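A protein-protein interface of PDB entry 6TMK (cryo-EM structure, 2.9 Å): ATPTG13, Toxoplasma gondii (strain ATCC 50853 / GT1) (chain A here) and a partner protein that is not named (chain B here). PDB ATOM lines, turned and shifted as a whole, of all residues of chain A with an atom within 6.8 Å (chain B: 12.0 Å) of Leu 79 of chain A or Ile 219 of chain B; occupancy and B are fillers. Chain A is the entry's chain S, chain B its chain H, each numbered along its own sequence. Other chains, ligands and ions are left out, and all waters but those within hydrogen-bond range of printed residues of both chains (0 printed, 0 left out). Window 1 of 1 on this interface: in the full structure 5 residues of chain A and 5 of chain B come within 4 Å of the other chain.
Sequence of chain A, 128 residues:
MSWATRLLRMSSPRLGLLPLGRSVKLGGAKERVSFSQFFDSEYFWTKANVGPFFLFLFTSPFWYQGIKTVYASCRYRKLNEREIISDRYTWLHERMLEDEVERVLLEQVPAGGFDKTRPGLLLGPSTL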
ATOM      1  N   CYS A  74      -1.281 -26.438  -8.004  1.00  0.00           N
ATOM      2  CA  CYS A  74      -2.285 -26.842  -8.987  1.00  0.00           C
ATOM      3  C   CYS A  74      -1.706 -26.822 -10.400  1.00  0.00           C
ATOM      4  O   CYS A  74      -1.857 -27.785 -11.174  1.00  0.00           O
ATOM      5  CB  CYS A  74      -3.497 -25.925  -8.879  1.00  0.00           C
ATOM      6  SG  CYS A  74      -4.456 -26.160  -7.373  1.00  0.00           S
ATOM      7  N   ARG A  75      -1.038 -25.722 -10.751  1.00  0.00           N
ATOM      8  CA  ARG A  75      -0.476 -25.584 -12.088  1.00  0.00           C
ATOM      9  C   ARG A  75       0.553 -26.667 -12.370  1.00  0.00           C
ATOM     10  O   ARG A  75       0.590 -27.223 -13.472  1.00  0.00           O
ATOM     11  CB  ARG A  75       0.134 -24.192 -12.243  1.00  0.00           C
ATOM     12  CG  ARG A  75       0.926 -23.968 -13.515  1.00  0.00           C
ATOM     13  CD  ARG A  75       0.099 -24.230 -14.747  1.00  0.00           C
ATOM     14  NE  ARG A  75      -1.056 -23.347 -14.827  1.00  0.00           N
ATOM     15  CZ  ARG A  75      -2.151 -23.614 -15.528  1.00  0.00           C
ATOM     16  NH1 ARG A  75      -2.248 -24.740 -16.214  1.00  0.00           N
ATOM     17  NH2 ARG A  75      -3.150 -22.753 -15.538  1.00  0.00           N
ATOM     18  N   TYR A  76       1.399 -26.978 -11.390  1.00  0.00           N
ATOM     19  CA  TYR A  76       2.445 -27.967 -11.589  1.00  0.00           C
ATOM     20  C   TYR A  76       1.859 -29.356 -11.758  1.00  0.00           C
ATOM     21  O   TYR A  76       2.376 -30.163 -12.533  1.00  0.00           O
ATOM     22  CB  TYR A  76       3.407 -27.941 -10.406  1.00  0.00           C
ATOM     23  CG  TYR A  76       4.537 -26.956 -10.541  1.00  0.00           C
ATOM     24  CD1 TYR A  76       5.853 -27.357 -10.414  1.00  0.00           C
ATOM     25  CD2 TYR A  76       4.286 -25.625 -10.793  1.00  0.00           C
ATOM     26  CE1 TYR A  76       6.882 -26.460 -10.537  1.00  0.00           C
ATOM     27  CE2 TYR A  76       5.306 -24.723 -10.916  1.00  0.00           C
ATOM     28  CZ  TYR A  76       6.602 -25.141 -10.784  1.00  0.00           C
ATOM     29  OH  TYR A  76       7.626 -24.239 -10.913  1.00  0.00           O
ATOM     30  N   ARG A  77       0.784 -29.659 -11.032  1.00  0.00           N
ATOM     31  CA  ARG A  77       0.101 -30.932 -11.227  1.00  0.00           C
ATOM     32  C   ARG A  77      -0.400 -31.065 -12.664  1.00  0.00           C
ATOM     33  O   ARG A  77      -0.124 -32.063 -13.355  1.00  0.00           O
ATOM     34  CB  ARG A  77      -1.047 -31.042 -10.232  1.00  0.00           C
ATOM     35  CG  ARG A  77      -1.348 -32.434  -9.773  1.00  0.00           C
ATOM     36  CD  ARG A  77      -2.368 -32.429  -8.663  1.00  0.00           C
ATOM     37  NE  ARG A  77      -1.742 -32.126  -7.377  1.00  0.00           N
ATOM     38  CZ  ARG A  77      -2.071 -31.109  -6.583  1.00  0.00           C
ATOM     39  NH1 ARG A  77      -3.032 -30.259  -6.910  1.00  0.00           N
ATOM     40  NH2 ARG A  77      -1.420 -30.940  -5.445  1.00  0.00           N
ATOM     41  N   LYS A  78      -1.145 -30.058 -13.130  1.00  0.00           N
ATOM     42  CA  LYS A  78      -1.639 -30.096 -14.503  1.00  0.00           C
ATOM     43  C   LYS A  78      -0.495 -30.213 -15.501  1.00  0.00           C
ATOM     44  O   LYS A  78      -0.587 -30.952 -16.491  1.00  0.00           O
ATOM     45  CB  LYS A  78      -2.468 -28.852 -14.799  1.00  0.00           C
ATOM     46  CG  LYS A  78      -3.742 -28.745 -14.003  1.00  0.00           C
ATOM     47  CD  LYS A  78      -4.468 -27.459 -14.338  1.00  0.00           C
ATOM     48  CE  LYS A  78      -5.400 -27.020 -13.227  1.00  0.00           C
ATOM     49  NZ  LYS A  78      -5.701 -25.564 -13.322  1.00  0.00           N
ATOM     50  N   LEU A  79       0.592 -29.488 -15.251  1.00  0.00           N
ATOM     51  CA  LEU A  79       1.718 -29.477 -16.170  1.00  0.00           C
ATOM     52  C   LEU A  79       2.406 -30.830 -16.218  1.00  0.00           C
ATOM     53  O   LEU A  79       2.852 -31.265 -17.281  1.00  0.00           O
ATOM     54  CB  LEU A  79       2.692 -28.383 -15.756  1.00  0.00           C
ATOM     55  CG  LEU A  79       4.006 -28.297 -16.511  1.00  0.00           C
ATOM     56  CD1 LEU A  79       3.780 -27.922 -17.949  1.00  0.00           C
ATOM     57  CD2 LEU A  79       4.855 -27.278 -15.828  1.00  0.00           C
ATOM     58  N   ASN A  80       2.529 -31.497 -15.073  1.00  0.00           N
ATOM     59  CA  ASN A  80       3.120 -32.826 -15.044  1.00  0.00           C
ATOM     60  C   ASN A  80       2.293 -33.796 -15.875  1.00  0.00           C
ATOM     61  O   ASN A  80       2.833 -34.581 -16.670  1.00  0.00           O
ATOM     62  CB  ASN A  80       3.217 -33.293 -13.595  1.00  0.00           C
ATOM     63  CG  ASN A  80       4.065 -34.521 -13.429  1.00  0.00           C
ATOM     64  OD1 ASN A  80       5.177 -34.603 -13.945  1.00  0.00           O
ATOM     65  ND2 ASN A  80       3.544 -35.487 -12.698  1.00  0.00           N
ATOM     66  N   GLU A  81       0.971 -33.749 -15.705  1.00  0.00           N
ATOM     67  CA  GLU A  81       0.090 -34.578 -16.523  1.00  0.00           C
ATOM     68  C   GLU A  81       0.320 -34.326 -18.011  1.00  0.00           C
ATOM     69  O   GLU A  81       0.529 -35.264 -18.800  1.00  0.00           O
ATOM     70  CB  GLU A  81      -1.362 -34.308 -16.148  1.00  0.00           C
ATOM     71  CG  GLU A  81      -2.354 -35.251 -16.770  1.00  0.00           C
ATOM     72  CD  GLU A  81      -3.711 -35.184 -16.105  1.00  0.00           C
ATOM     73  OE1 GLU A  81      -3.827 -35.625 -14.943  1.00  0.00           O
ATOM     74  OE2 GLU A  81      -4.662 -34.685 -16.741  1.00  0.00           O
ATOM     75  N   ARG A  82       0.291 -33.051 -18.407  1.00  0.00           N
ATOM     76  CA  ARG A  82       0.454 -32.706 -19.813  1.00  0.00           C
ATOM     77  C   ARG A  82       1.806 -33.156 -20.344  1.00  0.00           C
ATOM     78  O   ARG A  82       1.902 -33.649 -21.471  1.00  0.00           O
ATOM     79  CB  ARG A  82       0.280 -31.203 -20.006  1.00  0.00           C
ATOM     80  CG  ARG A  82       0.477 -30.751 -21.434  1.00  0.00           C
ATOM     81  CD  ARG A  82      -0.210 -29.443 -21.718  1.00  0.00           C
ATOM     82  NE  ARG A  82      -0.146 -29.102 -23.134  1.00  0.00           N
ATOM     83  CZ  ARG A  82      -0.390 -27.894 -23.622  1.00  0.00           C
ATOM     84  NH1 ARG A  82      -0.713 -26.902 -22.811  1.00  0.00           N
ATOM     85  NH2 ARG A  82      -0.306 -27.677 -24.923  1.00  0.00           N
ATOM     86  N   GLU A  83       2.861 -32.992 -19.551  1.00  0.00           N
ATOM     87  CA  GLU A  83       4.195 -33.356 -20.003  1.00  0.00           C
ATOM     88  C   GLU A  83       4.309 -34.855 -20.226  1.00  0.00           C
ATOM     89  O   GLU A  83       4.884 -35.300 -21.229  1.00  0.00           O
ATOM     90  CB  GLU A  83       5.227 -32.889 -18.980  1.00  0.00           C
ATOM     91  CG  GLU A  83       6.638 -32.828 -19.515  1.00  0.00           C
ATOM     92  CD  GLU A  83       7.695 -32.921 -18.429  1.00  0.00           C
ATOM     93  OE1 GLU A  83       7.386 -33.414 -17.325  1.00  0.00           O
ATOM     94  OE2 GLU A  83       8.845 -32.503 -18.685  1.00  0.00           O
ATOM     95  N   ILE A  84       3.770 -35.651 -19.304  1.00  0.00           N
ATOM     96  CA  ILE A  84       3.804 -37.100 -19.479  1.00  0.00           C
ATOM     97  C   ILE A  84       3.087 -37.494 -20.764  1.00  0.00           C
ATOM     98  O   ILE A  84       3.616 -38.257 -21.588  1.00  0.00           O
ATOM     99  CB  ILE A  84       3.196 -37.802 -18.253  1.00  0.00           C
ATOM    100  CG1 ILE A  84       4.085 -37.587 -17.040  1.00  0.00           C
ATOM    101  CG2 ILE A  84       3.038 -39.266 -18.513  1.00  0.00           C
ATOM    102  CD1 ILE A  84       3.421 -37.829 -15.751  1.00  0.00           C
ATOM    103  N   GLY B 215      14.141 -32.658 -28.302  1.00  0.00           N
ATOM    104  CA  GLY B 215      13.936 -31.719 -27.226  1.00  0.00           C
ATOM    105  C   GLY B 215      13.553 -32.387 -25.929  1.00  0.00           C
ATOM    106  O   GLY B 215      12.406 -32.806 -25.745  1.00  0.00           O
ATOM    107  N   TYR B 216      14.506 -32.472 -25.011  1.00  0.00           N
ATOM    108  CA  TYR B 216      14.293 -33.079 -23.708  1.00  0.00           C
ATOM    109  C   TYR B 216      14.558 -32.014 -22.662  1.00  0.00           C
ATOM    110  O   TYR B 216      15.636 -31.412 -22.643  1.00  0.00           O
ATOM    111  CB  TYR B 216      15.204 -34.286 -23.482  1.00  0.00           C
ATOM    112  CG  TYR B 216      14.892 -35.504 -24.312  1.00  0.00           C
ATOM    113  CD1 TYR B 216      13.604 -35.784 -24.719  1.00  0.00           C
ATOM    114  CD2 TYR B 216      15.892 -36.387 -24.667  1.00  0.00           C
ATOM    115  CE1 TYR B 216      13.326 -36.896 -25.469  1.00  0.00           C
ATOM    116  CE2 TYR B 216      15.622 -37.500 -25.413  1.00  0.00           C
ATOM    117  CZ  TYR B 216      14.339 -37.753 -25.810  1.00  0.00           C
ATOM    118  OH  TYR B 216      14.074 -38.872 -26.559  1.00  0.00           O
ATOM    119  N   ASN B 217      13.578 -31.785 -21.801  1.00  0.00           N
ATOM    120  CA  ASN B 217      13.703 -30.817 -20.732  1.00  0.00           C
ATOM    121  C   ASN B 217      12.918 -31.332 -19.541  1.00  0.00           C
ATOM    122  O   ASN B 217      12.271 -32.379 -19.600  1.00  0.00           O
ATOM    123  CB  ASN B 217      13.215 -29.442 -21.180  1.00  0.00           C
ATOM    124  CG  ASN B 217      13.872 -28.323 -20.427  1.00  0.00           C
ATOM    125  OD1 ASN B 217      14.160 -28.442 -19.241  1.00  0.00           O
ATOM    126  ND2 ASN B 217      14.112 -27.223 -21.109  1.00  0.00           N
ATOM    127  N   TYR B 218      12.983 -30.584 -18.451  1.00  0.00           N
ATOM    128  CA  TYR B 218      12.351 -30.987 -17.211  1.00  0.00           C
ATOM    129  C   TYR B 218      11.736 -29.774 -16.541  1.00  0.00           C
ATOM    130  O   TYR B 218      12.157 -28.638 -16.766  1.00  0.00           O
ATOM    131  CB  TYR B 218      13.345 -31.675 -16.271  1.00  0.00           C
ATOM    132  CG  TYR B 218      14.539 -30.844 -15.900  1.00  0.00           C
ATOM    133  CD1 TYR B 218      14.582 -30.163 -14.703  1.00  0.00           C
ATOM    134  CD2 TYR B 218      15.628 -30.746 -16.743  1.00  0.00           C
ATOM    135  CE1 TYR B 218      15.666 -29.406 -14.359  1.00  0.00           C
ATOM    136  CE2 TYR B 218      16.712 -29.992 -16.409  1.00  0.00           C
ATOM    137  CZ  TYR B 218      16.730 -29.319 -15.216  1.00  0.00           C
ATOM    138  OH  TYR B 218      17.825 -28.561 -14.881  1.00  0.00           O
ATOM    139  N   ILE B 219      10.718 -30.032 -15.727  1.00  0.00           N
ATOM    140  CA  ILE B 219      10.061 -28.975 -14.970  1.00  0.00           C
ATOM    141  C   ILE B 219      11.007 -28.558 -13.851  1.00  0.00           C
ATOM    142  O   ILE B 219      11.262 -29.328 -12.923  1.00  0.00           O
ATOM    143  CB  ILE B 219       8.712 -29.437 -14.414  1.00  0.00           C
ATOM    144  CG1 ILE B 219       7.714 -29.666 -15.537  1.00  0.00           C
ATOM    145  CG2 ILE B 219       8.146 -28.413 -13.488  1.00  0.00           C
ATOM    146  CD1 ILE B 219       6.686 -30.685 -15.202  1.00  0.00           C
ATOM    147  N   GLU B 220      11.542 -27.349 -13.944  1.00  0.00           N
ATOM    148  CA  GLU B 220      12.357 -26.803 -12.873  1.00  0.00           C
ATOM    149  C   GLU B 220      11.477 -26.300 -11.742  1.00  0.00           C
ATOM    150  O   GLU B 220      10.394 -25.756 -11.971  1.00  0.00           O
ATOM    151  CB  GLU B 220      13.234 -25.671 -13.397  1.00  0.00           C
ATOM    152  CG  GLU B 220      14.422 -26.136 -14.194  1.00  0.00           C
ATOM    153  CD  GLU B 220      15.372 -25.012 -14.529  1.00  0.00           C
ATOM    154  OE1 GLU B 220      15.375 -23.999 -13.798  1.00  0.00           O
ATOM    155  OE2 GLU B 220      16.117 -25.138 -15.523  1.00  0.00           O
ATOM    156  N   ASP B 221      11.951 -26.482 -10.514  1.00  0.00           N
ATOM    157  CA  ASP B 221      11.200 -26.043  -9.355  1.00  0.00           C
ATOM    158  C   ASP B 221      11.352 -24.542  -9.156  1.00  0.00           C
ATOM    159  O   ASP B 221      12.242 -23.895  -9.710  1.00  0.00           O
ATOM    160  CB  ASP B 221      11.657 -26.777  -8.099  1.00  0.00           C
ATOM    161  CG  ASP B 221      10.657 -26.666  -6.965  1.00  0.00           C
ATOM    162  OD1 ASP B 221       9.527 -26.196  -7.210  1.00  0.00           O
ATOM    163  OD2 ASP B 221      10.999 -27.042  -5.825  1.00  0.00           O
ATOM    164  N   ARG B 222      10.453 -23.990  -8.350  1.00  0.00           N
ATOM    165  CA  ARG B 222      10.527 -22.585  -8.017  1.00  0.00           C
ATOM    166  C   ARG B 222      11.839 -22.274  -7.309  1.00  0.00           C
ATOM    167  O   ARG B 222      12.556 -23.155  -6.833  1.00  0.00           O
ATOM    168  CB  ARG B 222       9.348 -22.185  -7.141  1.00  0.00           C
ATOM    169  CG  ARG B 222       8.007 -22.362  -7.795  1.00  0.00           C
ATOM    170  CD  ARG B 222       6.904 -22.310  -6.781  1.00  0.00           C
ATOM    171  NE  ARG B 222       6.649 -20.951  -6.321  1.00  0.00           N
ATOM    172  CZ  ARG B 222       6.196 -20.647  -5.111  1.00  0.00           C
ATOM    173  NH1 ARG B 222       5.948 -21.601  -4.226  1.00  0.00           N
ATOM    174  NH2 ARG B 222       5.999 -19.380  -4.784  1.00  0.00           N
ATOM    175  N   ARG B 223      12.134 -20.985  -7.230  1.00  0.00           N
ATOM    176  CA  ARG B 223      13.385 -20.542  -6.645  1.00  0.00           C
ATOM    177  C   ARG B 223      13.374 -20.769  -5.141  1.00  0.00           C
ATOM    178  O   ARG B 223      12.345 -20.614  -4.480  1.00  0.00           O
ATOM    179  CB  ARG B 223      13.609 -19.074  -6.974  1.00  0.00           C
ATOM    180  CG  ARG B 223      15.036 -18.645  -6.890  1.00  0.00           C
ATOM    181  CD  ARG B 223      15.215 -17.245  -7.413  1.00  0.00           C
ATOM    182  NE  ARG B 223      16.333 -16.568  -6.774  1.00  0.00           N
ATOM    183  CZ  ARG B 223      17.051 -15.612  -7.347  1.00  0.00           C
ATOM    184  NH1 ARG B 223      16.773 -15.210  -8.580  1.00  0.00           N
ATOM    185  NH2 ARG B 223      18.055 -15.060  -6.688  1.00  0.00           N
ATOM    186  N   SER B 239      21.640 -19.929 -17.408  1.00  0.00           N
ATOM    187  CA  SER B 239      20.688 -20.485 -18.354  1.00  0.00           C
ATOM    188  C   SER B 239      20.040 -21.760 -17.825  1.00  0.00           C
ATOM    189  O   SER B 239      18.902 -22.078 -18.171  1.00  0.00           O
ATOM    190  CB  SER B 239      21.398 -20.769 -19.672  1.00  0.00           C
ATOM    191  OG  SER B 239      22.059 -19.609 -20.140  1.00  0.00           O
ATOM    192  OXT SER B 239      20.631 -22.496 -17.036  1.00  0.00           O
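The side-chain hydroxyl (OH) of Tyr 76 of chain A lies within hydrogen-bond range of the backbone carbonyl oxygen (O) of Glu 220 of chain B, at 3.3 Å.
Among the printed residues, merely in contact across the chains: Tyr 76 of chain A with Ile 219 of chain B (3.8 Å), Tyr 76 of chain A with Arg 222 of chain B (3.7 Å), Leu 79 of chain A with Ile 219 of chain B (3.7 Å), Glu 83 of chain A with Asn 217 of chain B (3.5 Å) and Glu 83 of chain A with Ile 219 of chain B (3.5 Å).
Printed residues of chain B within 4 Å of Leu 79 of chain A: Ile 219 (3.7 Å). Ile 219 of chain B touches just these residues of chain A: Tyr 76, Leu 79 and Glu 83. No residue of chain B comes within 4 Å of Lys 78 of chain A. No residue of chain B comes within 4 Å of Asn 80 of chain A. Of chain B, only Asn 217 (3.5 Å) and Ile 219 (3.5 Å) come within 4 Å of Glu 83 of chain A. Printed residues of chain A within 4 Å of Glu 220 of chain B: Tyr 76 (3.3 Å). Of the printed residues of chain A, Arg 222 of chain B touches Tyr 76. Tyr 218 of chain B touches none of the printed residues of chain A. The nearest residue of chain A that does not touch Ile 219 of chain B is Asn 80 of chain A (4.2 Å).
Of the 10 printed residues of chain B, 4 touch a printed residue of chain A. Along chain B the printed residues that touch a printed residue of chain A span positions 217 to 222. Along chain A the printed residues that touch a printed residue of chain B span positions 76 to 83. Among the printed residues, no Asp or Glu carboxylate lies within 4 Å of a Lys or Arg side-chain nitrogen of the other chain.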
